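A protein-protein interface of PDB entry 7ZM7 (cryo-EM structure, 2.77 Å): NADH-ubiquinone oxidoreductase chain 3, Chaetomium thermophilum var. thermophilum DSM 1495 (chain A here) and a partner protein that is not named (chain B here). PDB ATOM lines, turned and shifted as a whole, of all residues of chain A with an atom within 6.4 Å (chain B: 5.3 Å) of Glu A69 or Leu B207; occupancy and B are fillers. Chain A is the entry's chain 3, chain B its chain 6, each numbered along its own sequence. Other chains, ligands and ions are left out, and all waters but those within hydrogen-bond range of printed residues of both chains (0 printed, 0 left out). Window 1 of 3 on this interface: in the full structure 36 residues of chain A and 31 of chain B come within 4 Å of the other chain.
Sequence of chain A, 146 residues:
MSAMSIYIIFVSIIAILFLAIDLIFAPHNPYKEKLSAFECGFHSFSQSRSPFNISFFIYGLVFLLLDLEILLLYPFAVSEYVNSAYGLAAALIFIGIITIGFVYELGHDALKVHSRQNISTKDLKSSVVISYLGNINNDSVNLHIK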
ATOM      1  N   PHE A  63      34.844 -18.227 -13.097  1.00  0.00           N
ATOM      2  CA  PHE A  63      33.732 -18.324 -12.166  1.00  0.00           C
ATOM      3  C   PHE A  63      32.917 -17.039 -12.164  1.00  0.00           C
ATOM      4  O   PHE A  63      31.700 -17.065 -12.337  1.00  0.00           O
ATOM      5  CB  PHE A  63      34.279 -18.631 -10.780  1.00  0.00           C
ATOM      6  CG  PHE A  63      33.289 -18.506  -9.684  1.00  0.00           C
ATOM      7  CD1 PHE A  63      32.162 -19.273  -9.664  1.00  0.00           C
ATOM      8  CD2 PHE A  63      33.496 -17.632  -8.660  1.00  0.00           C
ATOM      9  CE1 PHE A  63      31.257 -19.168  -8.649  1.00  0.00           C
ATOM     10  CE2 PHE A  63      32.587 -17.526  -7.645  1.00  0.00           C
ATOM     11  CZ  PHE A  63      31.475 -18.302  -7.636  1.00  0.00           C
ATOM     12  N   LEU A  64      33.586 -15.901 -12.011  1.00  0.00           N
ATOM     13  CA  LEU A  64      32.893 -14.630 -11.870  1.00  0.00           C
ATOM     14  C   LEU A  64      31.984 -14.348 -13.055  1.00  0.00           C
ATOM     15  O   LEU A  64      30.906 -13.772 -12.898  1.00  0.00           O
ATOM     16  CB  LEU A  64      33.916 -13.510 -11.711  1.00  0.00           C
ATOM     17  CG  LEU A  64      33.369 -12.096 -11.652  1.00  0.00           C
ATOM     18  CD1 LEU A  64      32.920 -11.792 -10.260  1.00  0.00           C
ATOM     19  CD2 LEU A  64      34.387 -11.110 -12.123  1.00  0.00           C
ATOM     20  N   LEU A  65      32.397 -14.743 -14.249  1.00  0.00           N
ATOM     21  CA  LEU A  65      31.596 -14.424 -15.416  1.00  0.00           C
ATOM     22  C   LEU A  65      30.474 -15.430 -15.605  1.00  0.00           C
ATOM     23  O   LEU A  65      29.314 -15.041 -15.734  1.00  0.00           O
ATOM     24  CB  LEU A  65      32.488 -14.337 -16.653  1.00  0.00           C
ATOM     25  CG  LEU A  65      33.509 -13.205 -16.609  1.00  0.00           C
ATOM     26  CD1 LEU A  65      34.321 -13.180 -17.882  1.00  0.00           C
ATOM     27  CD2 LEU A  65      32.848 -11.876 -16.367  1.00  0.00           C
ATOM     28  N   LEU A  66      30.793 -16.726 -15.578  1.00  0.00           N
ATOM     29  CA  LEU A  66      29.764 -17.759 -15.673  1.00  0.00           C
ATOM     30  C   LEU A  66      28.754 -17.672 -14.536  1.00  0.00           C
ATOM     31  O   LEU A  66      27.564 -17.925 -14.738  1.00  0.00           O
ATOM     32  CB  LEU A  66      30.406 -19.142 -15.687  1.00  0.00           C
ATOM     33  CG  LEU A  66      30.869 -19.786 -16.989  1.00  0.00           C
ATOM     34  CD1 LEU A  66      29.686 -20.011 -17.881  1.00  0.00           C
ATOM     35  CD2 LEU A  66      31.885 -18.952 -17.694  1.00  0.00           C
ATOM     36  N   ASP A  67      29.211 -17.347 -13.329  1.00  0.00           N
ATOM     37  CA  ASP A  67      28.307 -17.209 -12.189  1.00  0.00           C
ATOM     38  C   ASP A  67      27.346 -16.041 -12.377  1.00  0.00           C
ATOM     39  O   ASP A  67      26.175 -16.129 -12.010  1.00  0.00           O
ATOM     40  CB  ASP A  67      29.148 -17.073 -10.914  1.00  0.00           C
ATOM     41  CG  ASP A  67      28.343 -17.065  -9.653  1.00  0.00           C
ATOM     42  OD1 ASP A  67      27.841 -18.131  -9.251  1.00  0.00           O
ATOM     43  OD2 ASP A  67      28.315 -16.019  -8.993  1.00  0.00           O
ATOM     44  N   LEU A  68      27.823 -14.940 -12.958  1.00  0.00           N
ATOM     45  CA  LEU A  68      26.936 -13.859 -13.378  1.00  0.00           C
ATOM     46  C   LEU A  68      26.001 -14.296 -14.504  1.00  0.00           C
ATOM     47  O   LEU A  68      24.880 -13.797 -14.611  1.00  0.00           O
ATOM     48  CB  LEU A  68      27.762 -12.649 -13.815  1.00  0.00           C
ATOM     49  CG  LEU A  68      28.106 -11.563 -12.796  1.00  0.00           C
ATOM     50  CD1 LEU A  68      29.195 -10.663 -13.325  1.00  0.00           C
ATOM     51  CD2 LEU A  68      26.892 -10.735 -12.435  1.00  0.00           C
ATOM     52  N   GLU A  69      26.453 -15.202 -15.366  1.00  0.00           N
ATOM     53  CA  GLU A  69      25.656 -15.631 -16.515  1.00  0.00           C
ATOM     54  C   GLU A  69      24.509 -16.544 -16.097  1.00  0.00           C
ATOM     55  O   GLU A  69      23.374 -16.366 -16.543  1.00  0.00           O
ATOM     56  CB  GLU A  69      26.574 -16.324 -17.517  1.00  0.00           C
ATOM     57  CG  GLU A  69      27.578 -15.391 -18.142  1.00  0.00           C
ATOM     58  CD  GLU A  69      28.525 -16.069 -19.096  1.00  0.00           C
ATOM     59  OE1 GLU A  69      28.492 -17.309 -19.194  1.00  0.00           O
ATOM     60  OE2 GLU A  69      29.349 -15.365 -19.710  1.00  0.00           O
ATOM     61  N   ILE A  70      24.786 -17.532 -15.239  1.00  0.00           N
ATOM     62  CA  ILE A  70      23.730 -18.396 -14.715  1.00  0.00           C
ATOM     63  C   ILE A  70      22.755 -17.601 -13.862  1.00  0.00           C
ATOM     64  O   ILE A  70      21.558 -17.892 -13.840  1.00  0.00           O
ATOM     65  CB  ILE A  70      24.328 -19.590 -13.938  1.00  0.00           C
ATOM     66  CG1 ILE A  70      25.225 -20.436 -14.836  1.00  0.00           C
ATOM     67  CG2 ILE A  70      23.245 -20.478 -13.334  1.00  0.00           C
ATOM     68  CD1 ILE A  70      24.484 -21.035 -16.006  1.00  0.00           C
ATOM     69  N   LEU A  71      23.247 -16.596 -13.142  1.00  0.00           N
ATOM     70  CA  LEU A  71      22.361 -15.746 -12.357  1.00  0.00           C
ATOM     71  C   LEU A  71      21.311 -15.090 -13.241  1.00  0.00           C
ATOM     72  O   LEU A  71      20.148 -14.968 -12.852  1.00  0.00           O
ATOM     73  CB  LEU A  71      23.176 -14.689 -11.619  1.00  0.00           C
ATOM     74  CG  LEU A  71      22.446 -13.703 -10.699  1.00  0.00           C
ATOM     75  CD1 LEU A  71      22.290 -14.256  -9.295  1.00  0.00           C
ATOM     76  CD2 LEU A  71      23.127 -12.334 -10.692  1.00  0.00           C
ATOM     77  N   LEU A  72      21.706 -14.665 -14.438  1.00  0.00           N
ATOM     78  CA  LEU A  72      20.796 -14.014 -15.369  1.00  0.00           C
ATOM     79  C   LEU A  72      19.755 -14.958 -15.954  1.00  0.00           C
ATOM     80  O   LEU A  72      18.796 -14.488 -16.563  1.00  0.00           O
ATOM     81  CB  LEU A  72      21.599 -13.364 -16.490  1.00  0.00           C
ATOM     82  CG  LEU A  72      22.481 -12.210 -16.042  1.00  0.00           C
ATOM     83  CD1 LEU A  72      23.341 -11.726 -17.168  1.00  0.00           C
ATOM     84  CD2 LEU A  72      21.606 -11.096 -15.555  1.00  0.00           C
ATOM     85  N   LEU A  73      19.915 -16.264 -15.784  1.00  0.00           N
ATOM     86  CA  LEU A  73      18.959 -17.249 -16.268  1.00  0.00           C
ATOM     87  C   LEU A  73      17.948 -17.689 -15.219  1.00  0.00           C
ATOM     88  O   LEU A  73      16.887 -18.200 -15.582  1.00  0.00           O
ATOM     89  CB  LEU A  73      19.703 -18.474 -16.794  1.00  0.00           C
ATOM     90  CG  LEU A  73      20.140 -18.454 -18.249  1.00  0.00           C
ATOM     91  CD1 LEU A  73      20.844 -19.738 -18.577  1.00  0.00           C
ATOM     92  CD2 LEU A  73      18.948 -18.228 -19.186  1.00  0.00           C
ATOM     93  N   TYR A  74      18.250 -17.523 -13.935  1.00  0.00           N
ATOM     94  CA  TYR A  74      17.287 -17.888 -12.900  1.00  0.00           C
ATOM     95  C   TYR A  74      15.956 -17.168 -13.023  1.00  0.00           C
ATOM     96  O   TYR A  74      14.931 -17.786 -12.691  1.00  0.00           O
ATOM     97  CB  TYR A  74      17.875 -17.667 -11.503  1.00  0.00           C
ATOM     98  CG  TYR A  74      18.659 -18.839 -10.990  1.00  0.00           C
ATOM     99  CD1 TYR A  74      19.942 -19.083 -11.439  1.00  0.00           C
ATOM    100  CD2 TYR A  74      18.098 -19.732 -10.095  1.00  0.00           C
ATOM    101  CE1 TYR A  74      20.652 -20.145 -10.998  1.00  0.00           C
ATOM    102  CE2 TYR A  74      18.805 -20.820  -9.650  1.00  0.00           C
ATOM    103  CZ  TYR A  74      20.091 -21.015 -10.110  1.00  0.00           C
ATOM    104  OH  TYR A  74      20.838 -22.076  -9.680  1.00  0.00           O
ATOM    105  N   PHE A  94      20.650 -15.948 -25.673  1.00  0.00           N
ATOM    106  CA  PHE A  94      21.552 -15.559 -24.596  1.00  0.00           C
ATOM    107  C   PHE A  94      22.398 -16.733 -24.126  1.00  0.00           C
ATOM    108  O   PHE A  94      23.577 -16.565 -23.809  1.00  0.00           O
ATOM    109  CB  PHE A  94      20.780 -14.961 -23.427  1.00  0.00           C
ATOM    110  CG  PHE A  94      21.638 -14.676 -22.245  1.00  0.00           C
ATOM    111  CD1 PHE A  94      22.550 -13.645 -22.273  1.00  0.00           C
ATOM    112  CD2 PHE A  94      21.566 -15.454 -21.112  1.00  0.00           C
ATOM    113  CE1 PHE A  94      23.353 -13.393 -21.197  1.00  0.00           C
ATOM    114  CE2 PHE A  94      22.375 -15.188 -20.037  1.00  0.00           C
ATOM    115  CZ  PHE A  94      23.265 -14.159 -20.088  1.00  0.00           C
ATOM    116  N   ILE A  98      26.843 -16.977 -24.520  1.00  0.00           N
ATOM    117  CA  ILE A  98      27.749 -17.229 -23.409  1.00  0.00           C
ATOM    118  C   ILE A  98      28.347 -18.617 -23.507  1.00  0.00           C
ATOM    119  O   ILE A  98      29.317 -18.925 -22.811  1.00  0.00           O
ATOM    120  CB  ILE A  98      27.049 -17.036 -22.052  1.00  0.00           C
ATOM    121  CG1 ILE A  98      25.684 -17.703 -22.025  1.00  0.00           C
ATOM    122  CG2 ILE A  98      26.815 -15.565 -21.807  1.00  0.00           C
ATOM    123  CD1 ILE A  98      25.083 -17.810 -20.644  1.00  0.00           C
ATOM    124  N   THR A  99      27.779 -19.474 -24.344  1.00  0.00           N
ATOM    125  CA  THR A  99      28.389 -20.764 -24.626  1.00  0.00           C
ATOM    126  C   THR A  99      29.596 -20.633 -25.546  1.00  0.00           C
ATOM    127  O   THR A  99      30.601 -21.321 -25.361  1.00  0.00           O
ATOM    128  CB  THR A  99      27.345 -21.685 -25.234  1.00  0.00           C
ATOM    129  OG1 THR A  99      26.278 -21.851 -24.300  1.00  0.00           O
ATOM    130  CG2 THR A  99      27.940 -23.020 -25.561  1.00  0.00           C
ATOM    131  N   PHE A 102      32.540 -19.813 -23.722  1.00  0.00           N
ATOM    132  CA  PHE A 102      32.996 -20.967 -22.976  1.00  0.00           C
ATOM    133  C   PHE A 102      33.804 -21.929 -23.832  1.00  0.00           C
ATOM    134  O   PHE A 102      34.728 -22.567 -23.323  1.00  0.00           O
ATOM    135  CB  PHE A 102      31.792 -21.681 -22.364  1.00  0.00           C
ATOM    136  CG  PHE A 102      32.138 -22.936 -21.636  1.00  0.00           C
ATOM    137  CD1 PHE A 102      32.960 -22.894 -20.532  1.00  0.00           C
ATOM    138  CD2 PHE A 102      31.651 -24.161 -22.057  1.00  0.00           C
ATOM    139  CE1 PHE A 102      33.286 -24.040 -19.861  1.00  0.00           C
ATOM    140  CE2 PHE A 102      31.975 -25.298 -21.387  1.00  0.00           C
ATOM    141  CZ  PHE A 102      32.793 -25.237 -20.279  1.00  0.00           C
ATOM    142  N   LEU B 202      23.332  -6.809 -25.177  1.00  0.00           N
ATOM    143  CA  LEU B 202      24.528  -6.030 -24.883  1.00  0.00           C
ATOM    144  C   LEU B 202      25.284  -6.615 -23.710  1.00  0.00           C
ATOM    145  O   LEU B 202      26.518  -6.644 -23.709  1.00  0.00           O
ATOM    146  CB  LEU B 202      24.162  -4.581 -24.581  1.00  0.00           C
ATOM    147  CG  LEU B 202      23.730  -3.617 -25.686  1.00  0.00           C
ATOM    148  CD1 LEU B 202      22.787  -2.579 -25.098  1.00  0.00           C
ATOM    149  CD2 LEU B 202      24.904  -2.935 -26.309  1.00  0.00           C
ATOM    150  N   ALA B 203      24.560  -7.044 -22.677  1.00  0.00           N
ATOM    151  CA  ALA B 203      25.208  -7.603 -21.504  1.00  0.00           C
ATOM    152  C   ALA B 203      25.895  -8.919 -21.832  1.00  0.00           C
ATOM    153  O   ALA B 203      27.006  -9.178 -21.362  1.00  0.00           O
ATOM    154  CB  ALA B 203      24.190  -7.779 -20.392  1.00  0.00           C
ATOM    155  N   SER B 204      25.256  -9.756 -22.641  1.00  0.00           N
ATOM    156  CA  SER B 204      25.901 -10.977 -23.099  1.00  0.00           C
ATOM    157  C   SER B 204      27.206 -10.674 -23.810  1.00  0.00           C
ATOM    158  O   SER B 204      28.165 -11.446 -23.722  1.00  0.00           O
ATOM    159  CB  SER B 204      24.962 -11.738 -24.027  1.00  0.00           C
ATOM    160  OG  SER B 204      24.768 -11.013 -25.225  1.00  0.00           O
ATOM    161  N   PHE B 205      27.258  -9.566 -24.533  1.00  0.00           N
ATOM    162  CA  PHE B 205      28.466  -9.224 -25.254  1.00  0.00           C
ATOM    163  C   PHE B 205      29.513  -8.568 -24.361  1.00  0.00           C
ATOM    164  O   PHE B 205      30.705  -8.708 -24.632  1.00  0.00           O
ATOM    165  CB  PHE B 205      28.116  -8.343 -26.450  1.00  0.00           C
ATOM    166  CG  PHE B 205      27.750  -9.126 -27.674  1.00  0.00           C
ATOM    167  CD1 PHE B 205      28.724  -9.705 -28.457  1.00  0.00           C
ATOM    168  CD2 PHE B 205      26.435  -9.307 -28.027  1.00  0.00           C
ATOM    169  CE1 PHE B 205      28.394 -10.425 -29.573  1.00  0.00           C
ATOM    170  CE2 PHE B 205      26.097 -10.045 -29.137  1.00  0.00           C
ATOM    171  CZ  PHE B 205      27.079 -10.600 -29.912  1.00  0.00           C
ATOM    172  N   ILE B 206      29.099  -7.871 -23.300  1.00  0.00           N
ATOM    173  CA  ILE B 206      30.058  -7.293 -22.362  1.00  0.00           C
ATOM    174  C   ILE B 206      30.742  -8.393 -21.570  1.00  0.00           C
ATOM    175  O   ILE B 206      31.959  -8.370 -21.376  1.00  0.00           O
ATOM    176  CB  ILE B 206      29.371  -6.275 -21.432  1.00  0.00           C
ATOM    177  CG1 ILE B 206      29.091  -4.966 -22.161  1.00  0.00           C
ATOM    178  CG2 ILE B 206      30.218  -5.988 -20.220  1.00  0.00           C
ATOM    179  CD1 ILE B 206      28.334  -3.962 -21.339  1.00  0.00           C
ATOM    180  N   LEU B 207      29.968  -9.371 -21.098  1.00  0.00           N
ATOM    181  CA  LEU B 207      30.541 -10.511 -20.393  1.00  0.00           C
ATOM    182  C   LEU B 207      31.441 -11.331 -21.305  1.00  0.00           C
ATOM    183  O   LEU B 207      32.482 -11.835 -20.876  1.00  0.00           O
ATOM    184  CB  LEU B 207      29.424 -11.384 -19.829  1.00  0.00           C
ATOM    185  CG  LEU B 207      28.420 -10.743 -18.872  1.00  0.00           C
ATOM    186  CD1 LEU B 207      27.089 -11.471 -18.944  1.00  0.00           C
ATOM    187  CD2 LEU B 207      28.933 -10.752 -17.464  1.00  0.00           C
ATOM    188  N   LEU B 208      31.038 -11.500 -22.559  1.00  0.00           N
ATOM    189  CA  LEU B 208      31.836 -12.240 -23.524  1.00  0.00           C
ATOM    190  C   LEU B 208      33.151 -11.529 -23.834  1.00  0.00           C
ATOM    191  O   LEU B 208      34.171 -12.178 -24.075  1.00  0.00           O
ATOM    192  CB  LEU B 208      31.014 -12.449 -24.794  1.00  0.00           C
ATOM    193  CG  LEU B 208      31.670 -13.065 -26.014  1.00  0.00           C
ATOM    194  CD1 LEU B 208      32.001 -14.488 -25.725  1.00  0.00           C
ATOM    195  CD2 LEU B 208      30.738 -12.994 -27.164  1.00  0.00           C
ATOM    196  N   LEU B 209      33.139 -10.197 -23.862  1.00  0.00           N
ATOM    197  CA  LEU B 209      34.371  -9.446 -24.059  1.00  0.00           C
ATOM    198  C   LEU B 209      35.278  -9.534 -22.834  1.00  0.00           C
ATOM    199  O   LEU B 209      36.500  -9.632 -22.969  1.00  0.00           O
ATOM    200  CB  LEU B 209      34.046  -7.993 -24.398  1.00  0.00           C
ATOM    201  CG  LEU B 209      35.190  -6.976 -24.327  1.00  0.00           C
ATOM    202  CD1 LEU B 209      36.110  -7.130 -25.503  1.00  0.00           C
ATOM    203  CD2 LEU B 209      34.667  -5.552 -24.233  1.00  0.00           C
ATOM    204  N   ALA B 210      34.705  -9.498 -21.637  1.00  0.00           N
ATOM    205  CA  ALA B 210      35.495  -9.647 -20.429  1.00  0.00           C
ATOM    206  C   ALA B 210      36.072 -11.047 -20.282  1.00  0.00           C
ATOM    207  O   ALA B 210      37.006 -11.237 -19.506  1.00  0.00           O
ATOM    208  CB  ALA B 210      34.648  -9.281 -19.213  1.00  0.00           C
ATOM    209  N   MET B 211      35.528 -12.030 -20.994  1.00  0.00           N
ATOM    210  CA  MET B 211      36.137 -13.352 -21.033  1.00  0.00           C
ATOM    211  C   MET B 211      37.339 -13.366 -21.960  1.00  0.00           C
ATOM    212  O   MET B 211      38.458 -13.671 -21.546  1.00  0.00           O
ATOM    213  CB  MET B 211      35.113 -14.389 -21.483  1.00  0.00           C
ATOM    214  CG  MET B 211      35.676 -15.784 -21.652  1.00  0.00           C
ATOM    215  SD  MET B 211      35.774 -16.674 -20.091  1.00  0.00           S
ATOM    216  CE  MET B 211      34.111 -17.323 -19.982  1.00  0.00           C
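Hydrophobic or aromatic side chains of chain B that line the printed part of chain A: Leu B207 and Met B211.
Hydrophobic or aromatic side chains of chain A within 4 Å of the printed part of chain B: Leu A65, Leu A66 and Phe A94.
Among the printed residues, no Asp or Glu carboxylate lies within 4 Å of a Lys or Arg side-chain nitrogen of the other chain.
Printed residues of chain B within 4 Å of Leu A65: Leu B207 (3.8 Å), Ala B210 (3.7 Å) and Met B211 (3.5 Å).
Printed residues of chain B within 4 Å of Leu A66: Met B211.
Printed residues of chain B within 4 Å of Glu A69: Leu B207 (3.98 Å).
Printed residues of chain B within 4 Å of Phe A94: Ser B204 (3.5 Å).
Of the printed residues of chain A, Ser B204 touches Phe A94.
Printed residues of chain A within 4 Å of Leu B207: Leu A65 (3.8 Å) and Glu A69 (3.98 Å).
Of the printed residues of chain A, Met B211 touches Leu A65 (3.5 Å) and Leu A66 (3.6 Å).
The nearest printed residue of chain A that does not touch Leu B207 is Leu A68 (4.1 Å).
The nearest printed residue of chain A that does not touch Ser B204 is Ile A98 (4.7 Å).
Among the printed residues, merely in contact across the chains: Leu A65 with Met B211, Phe A94 with Ser B204, Leu A66 with Met B211, Leu A65 with Ala B210, Leu A65 with Leu B207 and Glu A69 with Leu B207.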
